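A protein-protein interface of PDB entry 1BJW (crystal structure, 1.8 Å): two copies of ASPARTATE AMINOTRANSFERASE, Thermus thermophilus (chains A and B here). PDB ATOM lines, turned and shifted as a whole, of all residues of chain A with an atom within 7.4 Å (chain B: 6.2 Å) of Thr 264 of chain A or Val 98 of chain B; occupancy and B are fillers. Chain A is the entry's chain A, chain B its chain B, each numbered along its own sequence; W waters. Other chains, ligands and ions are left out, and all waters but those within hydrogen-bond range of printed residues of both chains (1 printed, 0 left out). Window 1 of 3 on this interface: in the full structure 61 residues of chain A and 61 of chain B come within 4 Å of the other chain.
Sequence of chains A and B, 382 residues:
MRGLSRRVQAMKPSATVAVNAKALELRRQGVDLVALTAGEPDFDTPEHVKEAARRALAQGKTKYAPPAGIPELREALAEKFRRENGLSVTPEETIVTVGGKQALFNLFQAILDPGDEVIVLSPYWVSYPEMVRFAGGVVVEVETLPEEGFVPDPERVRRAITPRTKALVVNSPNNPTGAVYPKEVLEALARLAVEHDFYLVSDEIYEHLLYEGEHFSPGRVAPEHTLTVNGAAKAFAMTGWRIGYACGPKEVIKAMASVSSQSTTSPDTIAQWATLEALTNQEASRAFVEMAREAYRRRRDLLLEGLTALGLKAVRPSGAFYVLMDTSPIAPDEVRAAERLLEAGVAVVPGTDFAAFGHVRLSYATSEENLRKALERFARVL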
ATOM      1  N   TYR A  64      27.207  18.582  26.715  1.00  0.00           N
ATOM      2  CA  TYR A  64      26.625  19.700  27.468  1.00  0.00           C
ATOM      3  C   TYR A  64      27.673  20.762  27.829  1.00  0.00           C
ATOM      4  O   TYR A  64      28.835  20.452  28.123  1.00  0.00           O
ATOM      5  CB  TYR A  64      25.955  19.236  28.777  1.00  0.00           C
ATOM      6  CG  TYR A  64      24.643  18.484  28.641  1.00  0.00           C
ATOM      7  CD1 TYR A  64      23.539  19.039  27.970  1.00  0.00           C
ATOM      8  CD2 TYR A  64      24.487  17.254  29.240  1.00  0.00           C
ATOM      9  CE1 TYR A  64      22.309  18.373  27.917  1.00  0.00           C
ATOM     10  CE2 TYR A  64      23.274  16.577  29.198  1.00  0.00           C
ATOM     11  CZ  TYR A  64      22.190  17.135  28.542  1.00  0.00           C
ATOM     12  OH  TYR A  64      20.983  16.457  28.574  1.00  0.00           O
ATOM     13  N   PRO A  67      25.744  26.265  31.948  1.00  0.00           N
ATOM     14  CA  PRO A  67      24.552  27.103  31.768  1.00  0.00           C
ATOM     15  C   PRO A  67      24.791  28.542  31.304  1.00  0.00           C
ATOM     16  O   PRO A  67      23.959  29.096  30.599  1.00  0.00           O
ATOM     17  CB  PRO A  67      23.908  27.087  33.158  1.00  0.00           C
ATOM     18  CG  PRO A  67      24.395  25.809  33.776  1.00  0.00           C
ATOM     19  CD  PRO A  67      25.825  25.764  33.331  1.00  0.00           C
ATOM     20  N   VAL A  96      26.003  33.625  27.909  1.00  0.00           N
ATOM     21  CA  VAL A  96      25.676  33.205  26.538  1.00  0.00           C
ATOM     22  C   VAL A  96      24.271  32.598  26.594  1.00  0.00           C
ATOM     23  O   VAL A  96      24.008  31.717  27.426  1.00  0.00           O
ATOM     24  CB  VAL A  96      26.655  32.130  26.001  1.00  0.00           C
ATOM     25  CG1 VAL A  96      26.340  31.826  24.515  1.00  0.00           C
ATOM     26  CG2 VAL A  96      28.127  32.582  26.184  1.00  0.00           C
ATOM     27  N   THR A  97      23.397  33.030  25.681  1.00  0.00           N
ATOM     28  CA  THR A  97      22.000  32.593  25.655  1.00  0.00           C
ATOM     29  C   THR A  97      21.525  32.109  24.269  1.00  0.00           C
ATOM     30  O   THR A  97      22.246  32.229  23.293  1.00  0.00           O
ATOM     31  CB  THR A  97      21.065  33.753  26.153  1.00  0.00           C
ATOM     32  OG1 THR A  97      21.213  34.898  25.303  1.00  0.00           O
ATOM     33  CG2 THR A  97      21.408  34.155  27.606  1.00  0.00           C
ATOM     34  N   VAL A  98      20.327  31.530  24.213  1.00  0.00           N
ATOM     35  CA  VAL A  98      19.746  31.028  22.966  1.00  0.00           C
ATOM     36  C   VAL A  98      19.123  32.252  22.266  1.00  0.00           C
ATOM     37  O   VAL A  98      17.913  32.526  22.346  1.00  0.00           O
ATOM     38  CB  VAL A  98      18.753  29.856  23.253  1.00  0.00           C
ATOM     39  CG1 VAL A  98      18.105  29.365  21.983  1.00  0.00           C
ATOM     40  CG2 VAL A  98      19.520  28.696  23.917  1.00  0.00           C
ATOM     41  N   GLN A 102      16.435  35.298  24.251  1.00  0.00           N
ATOM     42  CA  GLN A 102      16.400  34.523  25.485  1.00  0.00           C
ATOM     43  C   GLN A 102      17.013  35.314  26.598  1.00  0.00           C
ATOM     44  O   GLN A 102      16.580  35.211  27.739  1.00  0.00           O
ATOM     45  CB  GLN A 102      17.086  33.156  25.384  1.00  0.00           C
ATOM     46  CG  GLN A 102      16.783  32.351  26.651  1.00  0.00           C
ATOM     47  CD  GLN A 102      17.612  31.114  26.846  1.00  0.00           C
ATOM     48  OE1 GLN A 102      18.771  31.049  26.508  1.00  0.00           O
ATOM     49  NE2 GLN A 102      16.996  30.118  27.430  1.00  0.00           N
ATOM     50  N   ASN A 106      14.957  35.772  30.005  1.00  0.00           N
ATOM     51  CA  ASN A 106      15.535  35.290  31.244  1.00  0.00           C
ATOM     52  C   ASN A 106      15.685  36.430  32.218  1.00  0.00           C
ATOM     53  O   ASN A 106      15.535  36.239  33.425  1.00  0.00           O
ATOM     54  CB  ASN A 106      16.886  34.650  30.975  1.00  0.00           C
ATOM     55  CG  ASN A 106      16.759  33.262  30.393  1.00  0.00           C
ATOM     56  OD1 ASN A 106      15.676  32.837  29.999  1.00  0.00           O
ATOM     57  ND2 ASN A 106      17.856  32.530  30.379  1.00  0.00           N
ATOM     58  N   ARG A 242      21.118  30.778  16.849  1.00  0.00           N
ATOM     59  CA  ARG A 242      20.602  31.031  18.213  1.00  0.00           C
ATOM     60  C   ARG A 242      21.666  31.264  19.333  1.00  0.00           C
ATOM     61  O   ARG A 242      21.751  30.518  20.313  1.00  0.00           O
ATOM     62  CB  ARG A 242      19.608  29.929  18.633  1.00  0.00           C
ATOM     63  CG  ARG A 242      18.580  29.522  17.553  1.00  0.00           C
ATOM     64  CD  ARG A 242      17.782  30.685  16.974  1.00  0.00           C
ATOM     65  NE  ARG A 242      17.104  31.489  18.000  1.00  0.00           N
ATOM     66  CZ  ARG A 242      17.312  32.786  18.181  1.00  0.00           C
ATOM     67  NH1 ARG A 242      18.168  33.432  17.406  1.00  0.00           N
ATOM     68  NH2 ARG A 242      16.703  33.431  19.158  1.00  0.00           N
ATOM     69  N   VAL A 259      17.959  30.618  35.389  1.00  0.00           N
ATOM     70  CA  VAL A 259      16.766  30.435  34.552  1.00  0.00           C
ATOM     71  C   VAL A 259      17.121  29.532  33.368  1.00  0.00           C
ATOM     72  O   VAL A 259      16.325  28.688  32.968  1.00  0.00           O
ATOM     73  CB  VAL A 259      16.170  31.779  34.012  1.00  0.00           C
ATOM     74  CG1 VAL A 259      14.923  31.499  33.155  1.00  0.00           C
ATOM     75  CG2 VAL A 259      15.738  32.673  35.181  1.00  0.00           C
ATOM     76  N   SER A 260      18.320  29.707  32.826  1.00  0.00           N
ATOM     77  CA  SER A 260      18.746  28.871  31.708  1.00  0.00           C
ATOM     78  C   SER A 260      18.877  27.422  32.132  1.00  0.00           C
ATOM     79  O   SER A 260      18.388  26.523  31.443  1.00  0.00           O
ATOM     80  CB  SER A 260      20.081  29.341  31.153  1.00  0.00           C
ATOM     81  OG  SER A 260      19.933  30.580  30.504  1.00  0.00           O
ATOM     82  N   SER A 261      19.466  27.196  33.308  1.00  0.00           N
ATOM     83  CA  SER A 261      19.673  25.827  33.780  1.00  0.00           C
ATOM     84  C   SER A 261      18.402  25.006  33.960  1.00  0.00           C
ATOM     85  O   SER A 261      18.452  23.789  33.855  1.00  0.00           O
ATOM     86  CB  SER A 261      20.546  25.806  35.039  1.00  0.00           C
ATOM     87  OG  SER A 261      19.855  26.407  36.099  1.00  0.00           O
ATOM     88  N   GLN A 262      17.265  25.653  34.201  1.00  0.00           N
ATOM     89  CA  GLN A 262      16.004  24.924  34.367  1.00  0.00           C
ATOM     90  C   GLN A 262      15.143  24.984  33.096  1.00  0.00           C
ATOM     91  O   GLN A 262      14.017  24.474  33.073  1.00  0.00           O
ATOM     92  CB  GLN A 262      15.151  25.527  35.475  1.00  0.00           C
ATOM     93  CG  GLN A 262      15.743  25.613  36.832  1.00  0.00           C
ATOM     94  CD  GLN A 262      14.928  26.581  37.687  1.00  0.00           C
ATOM     95  OE1 GLN A 262      15.441  27.610  38.130  1.00  0.00           O
ATOM     96  NE2 GLN A 262      13.630  26.287  37.865  1.00  0.00           N
ATOM     97  N   SER A 263      15.629  25.639  32.053  1.00  0.00           N
ATOM     98  CA  SER A 263      14.816  25.722  30.854  1.00  0.00           C
ATOM     99  C   SER A 263      15.471  25.149  29.572  1.00  0.00           C
ATOM    100  O   SER A 263      14.904  24.275  28.921  1.00  0.00           O
ATOM    101  CB  SER A 263      14.364  27.178  30.660  1.00  0.00           C
ATOM    102  OG  SER A 263      15.473  28.053  30.604  1.00  0.00           O
ATOM    103  N   THR A 264      16.677  25.604  29.259  1.00  0.00           N
ATOM    104  CA  THR A 264      17.378  25.167  28.045  1.00  0.00           C
ATOM    105  C   THR A 264      18.703  24.485  28.325  1.00  0.00           C
ATOM    106  O   THR A 264      19.323  23.900  27.428  1.00  0.00           O
ATOM    107  CB  THR A 264      17.678  26.407  27.138  1.00  0.00           C
ATOM    108  OG1 THR A 264      18.286  27.444  27.935  1.00  0.00           O
ATOM    109  CG2 THR A 264      16.379  26.939  26.490  1.00  0.00           C
ATOM    110  N   THR A 265      19.114  24.552  29.591  1.00  0.00           N
ATOM    111  CA  THR A 265      20.406  24.048  30.091  1.00  0.00           C
ATOM    112  C   THR A 265      21.543  24.972  29.624  1.00  0.00           C
ATOM    113  O   THR A 265      22.157  25.674  30.433  1.00  0.00           O
ATOM    114  CB  THR A 265      20.707  22.584  29.696  1.00  0.00           C
ATOM    115  OG1 THR A 265      19.618  21.766  30.116  1.00  0.00           O
ATOM    116  CG2 THR A 265      21.999  22.102  30.370  1.00  0.00           C
ATOM    117  N   SER A 266      21.766  25.022  28.310  1.00  0.00           N
ATOM    118  CA  SER A 266      22.800  25.856  27.714  1.00  0.00           C
ATOM    119  C   SER A 266      22.585  25.878  26.190  1.00  0.00           C
ATOM    120  O   SER A 266      21.960  24.953  25.647  1.00  0.00           O
ATOM    121  CB  SER A 266      24.178  25.242  27.987  1.00  0.00           C
ATOM    122  OG  SER A 266      25.212  26.144  27.621  1.00  0.00           O
ATOM    123  N   PRO A 267      23.067  26.940  25.493  1.00  0.00           N
ATOM    124  CA  PRO A 267      22.914  27.013  24.028  1.00  0.00           C
ATOM    125  C   PRO A 267      23.757  25.915  23.356  1.00  0.00           C
ATOM    126  O   PRO A 267      24.717  25.405  23.952  1.00  0.00           O
ATOM    127  CB  PRO A 267      23.474  28.406  23.689  1.00  0.00           C
ATOM    128  CG  PRO A 267      23.225  29.192  24.962  1.00  0.00           C
ATOM    129  CD  PRO A 267      23.621  28.208  26.024  1.00  0.00           C
ATOM    130  N   ASP A 268      23.390  25.541  22.129  1.00  0.00           N
ATOM    131  CA  ASP A 268      24.117  24.513  21.387  1.00  0.00           C
ATOM    132  C   ASP A 268      25.634  24.753  21.435  1.00  0.00           C
ATOM    133  O   ASP A 268      26.112  25.853  21.161  1.00  0.00           O
ATOM    134  CB  ASP A 268      23.598  24.436  19.937  1.00  0.00           C
ATOM    135  CG  ASP A 268      24.607  23.807  18.975  1.00  0.00           C
ATOM    136  OD1 ASP A 268      25.157  22.716  19.254  1.00  0.00           O
ATOM    137  OD2 ASP A 268      24.861  24.423  17.926  1.00  0.00           O
ATOM    138  N   VAL B  96       9.297  20.974  18.122  1.00  0.00           N
ATOM    139  CA  VAL B  96      10.732  20.858  18.322  1.00  0.00           C
ATOM    140  C   VAL B  96      11.115  21.950  19.339  1.00  0.00           C
ATOM    141  O   VAL B  96      10.657  23.087  19.239  1.00  0.00           O
ATOM    142  CB  VAL B  96      11.507  21.049  16.994  1.00  0.00           C
ATOM    143  CG1 VAL B  96      12.991  20.832  17.199  1.00  0.00           C
ATOM    144  CG2 VAL B  96      10.945  20.074  15.942  1.00  0.00           C
ATOM    145  N   THR B  97      11.974  21.586  20.290  1.00  0.00           N
ATOM    146  CA  THR B  97      12.411  22.483  21.355  1.00  0.00           C
ATOM    147  C   THR B  97      13.934  22.448  21.587  1.00  0.00           C
ATOM    148  O   THR B  97      14.655  21.613  21.047  1.00  0.00           O
ATOM    149  CB  THR B  97      11.659  22.116  22.702  1.00  0.00           C
ATOM    150  OG1 THR B  97      11.876  20.730  23.043  1.00  0.00           O
ATOM    151  CG2 THR B  97      10.158  22.347  22.539  1.00  0.00           C
ATOM    152  N   VAL B  98      14.413  23.365  22.421  1.00  0.00           N
ATOM    153  CA  VAL B  98      15.829  23.454  22.766  1.00  0.00           C
ATOM    154  C   VAL B  98      16.049  22.418  23.892  1.00  0.00           C
ATOM    155  O   VAL B  98      16.064  22.745  25.082  1.00  0.00           O
ATOM    156  CB  VAL B  98      16.219  24.910  23.209  1.00  0.00           C
ATOM    157  CG1 VAL B  98      17.670  24.983  23.567  1.00  0.00           C
ATOM    158  CG2 VAL B  98      15.985  25.920  22.043  1.00  0.00           C
ATOM    159  N   GLY B  99      16.183  21.163  23.475  1.00  0.00           N
ATOM    160  CA  GLY B  99      16.356  20.057  24.392  1.00  0.00           C
ATOM    161  C   GLY B  99      15.013  19.629  24.948  1.00  0.00           C
ATOM    162  O   GLY B  99      14.027  20.357  24.844  1.00  0.00           O
ATOM    163  N   GLY B 100      14.933  18.400  25.442  1.00  0.00           N
ATOM    164  CA  GLY B 100      13.696  17.960  26.059  1.00  0.00           C
ATOM    165  C   GLY B 100      13.399  18.808  27.306  1.00  0.00           C
ATOM    166  O   GLY B 100      12.241  18.920  27.724  1.00  0.00           O
ATOM    167  N   LYS B 101      14.430  19.379  27.929  1.00  0.00           N
ATOM    168  CA  LYS B 101      14.204  20.206  29.112  1.00  0.00           C
ATOM    169  C   LYS B 101      13.337  21.443  28.743  1.00  0.00           C
ATOM    170  O   LYS B 101      12.432  21.818  29.506  1.00  0.00           O
ATOM    171  CB  LYS B 101      15.520  20.653  29.741  1.00  0.00           C
ATOM    172  CG  LYS B 101      15.252  21.446  31.034  1.00  0.00           C
ATOM    173  CD  LYS B 101      16.505  21.944  31.682  1.00  0.00           C
ATOM    174  CE  LYS B 101      17.228  20.781  32.305  1.00  0.00           C
ATOM    175  NZ  LYS B 101      18.562  21.269  32.721  1.00  0.00           N
ATOM    176  N   GLN B 102      13.561  22.046  27.571  1.00  0.00           N
ATOM    177  CA  GLN B 102      12.727  23.185  27.197  1.00  0.00           C
ATOM    178  C   GLN B 102      11.285  22.783  26.914  1.00  0.00           C
ATOM    179  O   GLN B 102      10.372  23.561  27.166  1.00  0.00           O
ATOM    180  CB  GLN B 102      13.280  24.003  26.035  1.00  0.00           C
ATOM    181  CG  GLN B 102      12.477  25.303  25.919  1.00  0.00           C
ATOM    182  CD  GLN B 102      12.626  26.032  24.591  1.00  0.00           C
ATOM    183  OE1 GLN B 102      12.863  25.421  23.570  1.00  0.00           O
ATOM    184  NE2 GLN B 102      12.449  27.343  24.615  1.00  0.00           N
ATOM    185  N   ALA B 103      11.072  21.564  26.413  1.00  0.00           N
ATOM    186  CA  ALA B 103       9.724  21.069  26.180  1.00  0.00           C
ATOM    187  C   ALA B 103       8.976  20.985  27.538  1.00  0.00           C
ATOM    188  O   ALA B 103       7.816  21.370  27.657  1.00  0.00           O
ATOM    189  CB  ALA B 103       9.784  19.677  25.526  1.00  0.00           C
ATOM    190  N   PHE B 105       9.791  22.651  30.358  1.00  0.00           N
ATOM    191  CA  PHE B 105       9.668  24.018  30.880  1.00  0.00           C
ATOM    192  C   PHE B 105       8.493  24.740  30.225  1.00  0.00           C
ATOM    193  O   PHE B 105       7.654  25.340  30.907  1.00  0.00           O
ATOM    194  CB  PHE B 105      10.963  24.792  30.629  1.00  0.00           C
ATOM    195  CG  PHE B 105      10.911  26.235  31.062  1.00  0.00           C
ATOM    196  CD1 PHE B 105      10.484  27.227  30.172  1.00  0.00           C
ATOM    197  CD2 PHE B 105      11.313  26.601  32.346  1.00  0.00           C
ATOM    198  CE1 PHE B 105      10.458  28.561  30.560  1.00  0.00           C
ATOM    199  CE2 PHE B 105      11.301  27.935  32.761  1.00  0.00           C
ATOM    200  CZ  PHE B 105      10.872  28.920  31.870  1.00  0.00           C
ATOM    201  N1  LLP B 234      14.501  14.143  31.164  1.00  0.00           N
ATOM    202  C2  LLP B 234      15.485  13.329  31.716  1.00  0.00           C
ATOM    203  C2' LLP B 234      15.164  12.463  32.903  1.00  0.00           C
ATOM    204  C3  LLP B 234      16.745  13.342  31.202  1.00  0.00           C
ATOM    205  O3  LLP B 234      17.713  12.711  31.858  1.00  0.00           O
ATOM    206  C4  LLP B 234      17.007  14.168  30.101  1.00  0.00           C
ATOM    207  C4' LLP B 234      18.335  14.079  29.415  1.00  0.00           C
ATOM    208  C5  LLP B 234      15.968  14.951  29.564  1.00  0.00           C
ATOM    209  C6  LLP B 234      14.741  14.954  30.104  1.00  0.00           C
ATOM    210  C5' LLP B 234      16.157  15.931  28.411  1.00  0.00           C
ATOM    211  OP4 LLP B 234      17.507  16.329  28.068  1.00  0.00           O
ATOM    212  P   LLP B 234      17.889  17.459  26.972  1.00  0.00           P
ATOM    213  OP1 LLP B 234      17.206  16.964  25.800  1.00  0.00           O
ATOM    214  OP2 LLP B 234      19.379  17.327  26.900  1.00  0.00           O
ATOM    215  OP3 LLP B 234      17.443  18.768  27.492  1.00  0.00           O
ATOM    216  N   LLP B 234      19.868  11.718  24.466  1.00  0.00           N
ATOM    217  CA  LLP B 234      20.351  10.462  25.055  1.00  0.00           C
ATOM    218  CB  LLP B 234      19.460  10.078  26.250  1.00  0.00           C
ATOM    219  CG  LLP B 234      19.218  11.251  27.233  1.00  0.00           C
ATOM    220  CD  LLP B 234      20.539  11.689  27.948  1.00  0.00           C
ATOM    221  CE  LLP B 234      20.426  13.033  28.735  1.00  0.00           C
ATOM    222  NZ  LLP B 234      19.186  13.053  29.527  1.00  0.00           N
ATOM    223  C   LLP B 234      20.511   9.276  24.089  1.00  0.00           C
ATOM    224  O   LLP B 234      21.501   8.543  24.167  1.00  0.00           O
ATOM    225  N   ARG B 242      21.195  20.317  21.649  1.00  0.00           N
ATOM    226  CA  ARG B 242      19.979  20.949  22.212  1.00  0.00           C
ATOM    227  C   ARG B 242      18.707  20.809  21.345  1.00  0.00           C
ATOM    228  O   ARG B 242      18.102  21.811  20.921  1.00  0.00           O
ATOM    229  CB  ARG B 242      20.213  22.444  22.554  1.00  0.00           C
ATOM    230  CG  ARG B 242      21.480  22.788  23.352  1.00  0.00           C
ATOM    231  CD  ARG B 242      21.688  21.956  24.604  1.00  0.00           C
ATOM    232  NE  ARG B 242      20.560  22.022  25.516  1.00  0.00           N
ATOM    233  CZ  ARG B 242      19.935  20.945  25.995  1.00  0.00           C
ATOM    234  NH1 ARG B 242      20.327  19.721  25.639  1.00  0.00           N
ATOM    235  NH2 ARG B 242      18.913  21.094  26.823  1.00  0.00           N
ATOM    236  N   ILE B 243      18.334  19.566  21.041  1.00  0.00           N
ATOM    237  CA  ILE B 243      17.130  19.295  20.257  1.00  0.00           C
ATOM    238  C   ILE B 243      16.259  18.284  20.995  1.00  0.00           C
ATOM    239  O   ILE B 243      16.642  17.127  21.167  1.00  0.00           O
ATOM    240  CB  ILE B 243      17.422  18.720  18.820  1.00  0.00           C
ATOM    241  CG1 ILE B 243      18.115  19.759  17.930  1.00  0.00           C
ATOM    242  CG2 ILE B 243      16.103  18.273  18.201  1.00  0.00           C
ATOM    243  CD1 ILE B 243      17.225  20.944  17.529  1.00  0.00           C
ATOM    244  N   GLY B 244      15.087  18.747  21.410  1.00  0.00           N
ATOM    245  CA  GLY B 244      14.112  17.916  22.102  1.00  0.00           C
ATOM    246  C   GLY B 244      12.826  17.979  21.284  1.00  0.00           C
ATOM    247  O   GLY B 244      12.731  18.767  20.341  1.00  0.00           O
ATOM    248  N   THR B 264      12.867  31.761  22.969  1.00  0.00           N
ATOM    249  CA  THR B 264      14.018  31.325  22.185  1.00  0.00           C
ATOM    250  C   THR B 264      13.826  31.453  20.660  1.00  0.00           C
ATOM    251  O   THR B 264      14.792  31.298  19.892  1.00  0.00           O
ATOM    252  CB  THR B 264      14.293  29.843  22.512  1.00  0.00           C
ATOM    253  OG1 THR B 264      13.057  29.117  22.400  1.00  0.00           O
ATOM    254  CG2 THR B 264      14.818  29.698  23.936  1.00  0.00           C
ATOM    255  N   SER B 266      13.163  29.744  18.056  1.00  0.00           N
ATOM    256  CA  SER B 266      13.182  28.382  17.540  1.00  0.00           C
ATOM    257  C   SER B 266      14.573  27.789  17.766  1.00  0.00           C
ATOM    258  O   SER B 266      15.549  28.526  17.865  1.00  0.00           O
ATOM    259  CB  SER B 266      12.896  28.374  16.032  1.00  0.00           C
ATOM    260  OG  SER B 266      12.698  27.048  15.552  1.00  0.00           O
ATOM    261  N   PRO B 267      14.679  26.446  17.911  1.00  0.00           N
ATOM    262  CA  PRO B 267      16.011  25.852  18.115  1.00  0.00           C
ATOM    263  C   PRO B 267      16.930  26.099  16.903  1.00  0.00           C
ATOM    264  O   PRO B 267      16.455  26.362  15.807  1.00  0.00           O
ATOM    265  CB  PRO B 267      15.705  24.355  18.255  1.00  0.00           C
ATOM    266  CG  PRO B 267      14.285  24.298  18.719  1.00  0.00           C
ATOM    267  CD  PRO B 267      13.601  25.439  18.047  1.00  0.00           C
ATOM    268  N   ASP B 268      18.236  25.993  17.119  1.00  0.00           N
ATOM    269  CA  ASP B 268      19.279  26.163  16.098  1.00  0.00           C
ATOM    270  C   ASP B 268      18.854  25.416  14.808  1.00  0.00           C
ATOM    271  O   ASP B 268      18.583  24.203  14.821  1.00  0.00           O
ATOM    272  CB  ASP B 268      20.606  25.605  16.713  1.00  0.00           C
ATOM    273  CG  ASP B 268      21.782  25.580  15.742  1.00  0.00           C
ATOM    274  OD1 ASP B 268      21.673  24.985  14.668  1.00  0.00           O
ATOM    275  OD2 ASP B 268      22.865  26.128  16.073  1.00  0.00           O
HETATM  276  O   HOH W   1      18.937  19.022  29.970  1.00  0.00           O
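Water W1 lies within hydrogen-bond range of OG1 of Thr 265 of chain A (2.8 Å) and OP3 of LLP 234 of chain B (2.9 Å).
Of the printed residues of chain B, Arg 242 of chain A touches Thr 264, Ser 266, Pro 267 and Asp 268. Printed residues of chain B within 4 Å of Ser 263 of chain A: Lys 101, Gln 102 and Phe 105. Of chain B, only Val 98 (3.7 Å) and Arg 242 (2.9 Å) come within 4 Å of Thr 264 of chain A. Val 98 of chain B touches one residue of chain A. No residue of chain A comes within 4 Å of Gly 99 of chain B. The nearest residue of chain B that does not touch Thr 264 of chain A is Thr 264 of chain B (4.1 Å). The nearest printed residue of chain B that does not touch Gln 262 of chain A is Gln 102 of chain B (6.0 Å).
Of the 18 printed residues of chain A, 11 touch a printed residue of chain B. Of the 17 printed residues of chain B, 10 touch a printed residue of chain A. Hydrophobic or aromatic side chains of chain B that line the printed part of chain A: Val 98 and Phe 105.
Val 98 of chain A touches Thr 264 of chain B, and with the chains exchanged Thr 264 of chain A touches Val 98 of chain B. Arg 242 of chain A touches Pro 267 of chain B, and with the chains exchanged Pro 267 of chain A touches Arg 242 of chain B. Arg 242 of chain A touches Asp 268 of chain B, and with the chains exchanged Asp 268 of chain A touches Arg 242 of chain B. Asp 268 of chain B touches its own counterpart, Asp 268 of chain A. Of the 21 pairs that touch across the chains among the printed residues, 11 have their exchanged pair printed and touching as well.
O of Thr 264 of chain A sits at hydrogen-bond distance from NH2 of Arg 242 of chain B, 2.9 Å away. The side-chain hydroxyl (OH) of Tyr 64 of chain A sits at hydrogen-bond distance from OP2 of LLP 234 of chain B, 2.5 Å away. The side-chain hydroxyl (OG1) of Thr 265 of chain A lies within hydrogen-bond range of the side-chain amino group (NZ) of Lys 101 of chain B. The side-chain carboxylate of Asp 268 of chain A sits close to the side-chain carboxylate of Asp 268 of chain B, at 3.2 Å. The backbone carbonyl oxygen (O) of Ser 266 of chain B sits close to the guanidinium group (NE) of Arg 242 of chain A, at 3.3 Å. The guanidinium group (NH2) of Arg 242 of chain A lies within hydrogen-bond range of the backbone carbonyl oxygen (O) of Thr 264 of chain B. O of Ser 263 of chain A is in hydrogen-bond range of N of Gln 102 of chain B. O of Ser 266 of chain A sits close to NE of Arg 242 of chain B, 3.3 Å away. The backbone carbonyl oxygen (O) of Ser 261 of chain A is in hydrogen-bond range of the side-chain amino group (NZ) of Lys 101 of chain B. The side-chain hydroxyl of Thr 265 of chain A lies within hydrogen-bond range of the guanidinium group of Arg 242 of chain B.
The backbone carbonyl oxygen (O) of Val 259 of chain A lies within hydrogen-bond range of the side-chain hydroxyl (OG) of Ser 263 of chain A (2.6 Å). OG1 of Thr 264 of chain A is in hydrogen-bond range of NE2 of Gln 102 of chain A (3.0 Å). The side-chain hydroxyl (OG) of Ser 263 of chain A is in hydrogen-bond range of the backbone carbonyl oxygen (O) of Ser 260 of chain A. The backbone carbonyl oxygen (O) of Arg 242 of chain B sits at hydrogen-bond distance from the backbone NH (N) of Gly 99 of chain B (3.3 Å). The backbone NH (N) of Gly 100 of chain B sits at hydrogen-bond distance from OP1 of LLP 234 of chain B, 2.7 Å away. O of Ser 260 of chain A lies within hydrogen-bond range of N of Thr 265 of chain A, 2.8 Å away.
Arg 242 of chain B touches Tyr 64 of chain A. Thr 264 of chain B touches Val 98 of chain A. C of Pro 267 of chain B touches CG of Arg 242 of chain A, 3.9 Å away. Asp 268 of chain B touches Arg 242 of chain A (N to CG, 3.6 Å). Gln 262 of chain A touches Lys 101 of chain B (C to CD, 3.6 Å). Phe 105 of chain B touches Gln 262 of chain A (CD2 to O, 3.5 Å). Lys 101 of chain B touches Ser 263 of chain A (C to O, 3.2 Å). CB of Ser 263 of chain A touches CD2 of Phe 105 of chain B, at 3.5 Å. Thr 264 of chain A touches Val 98 of chain B. Arg 242 of chain B touches Asp 268 of chain A (CG to N, 3.6 Å).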
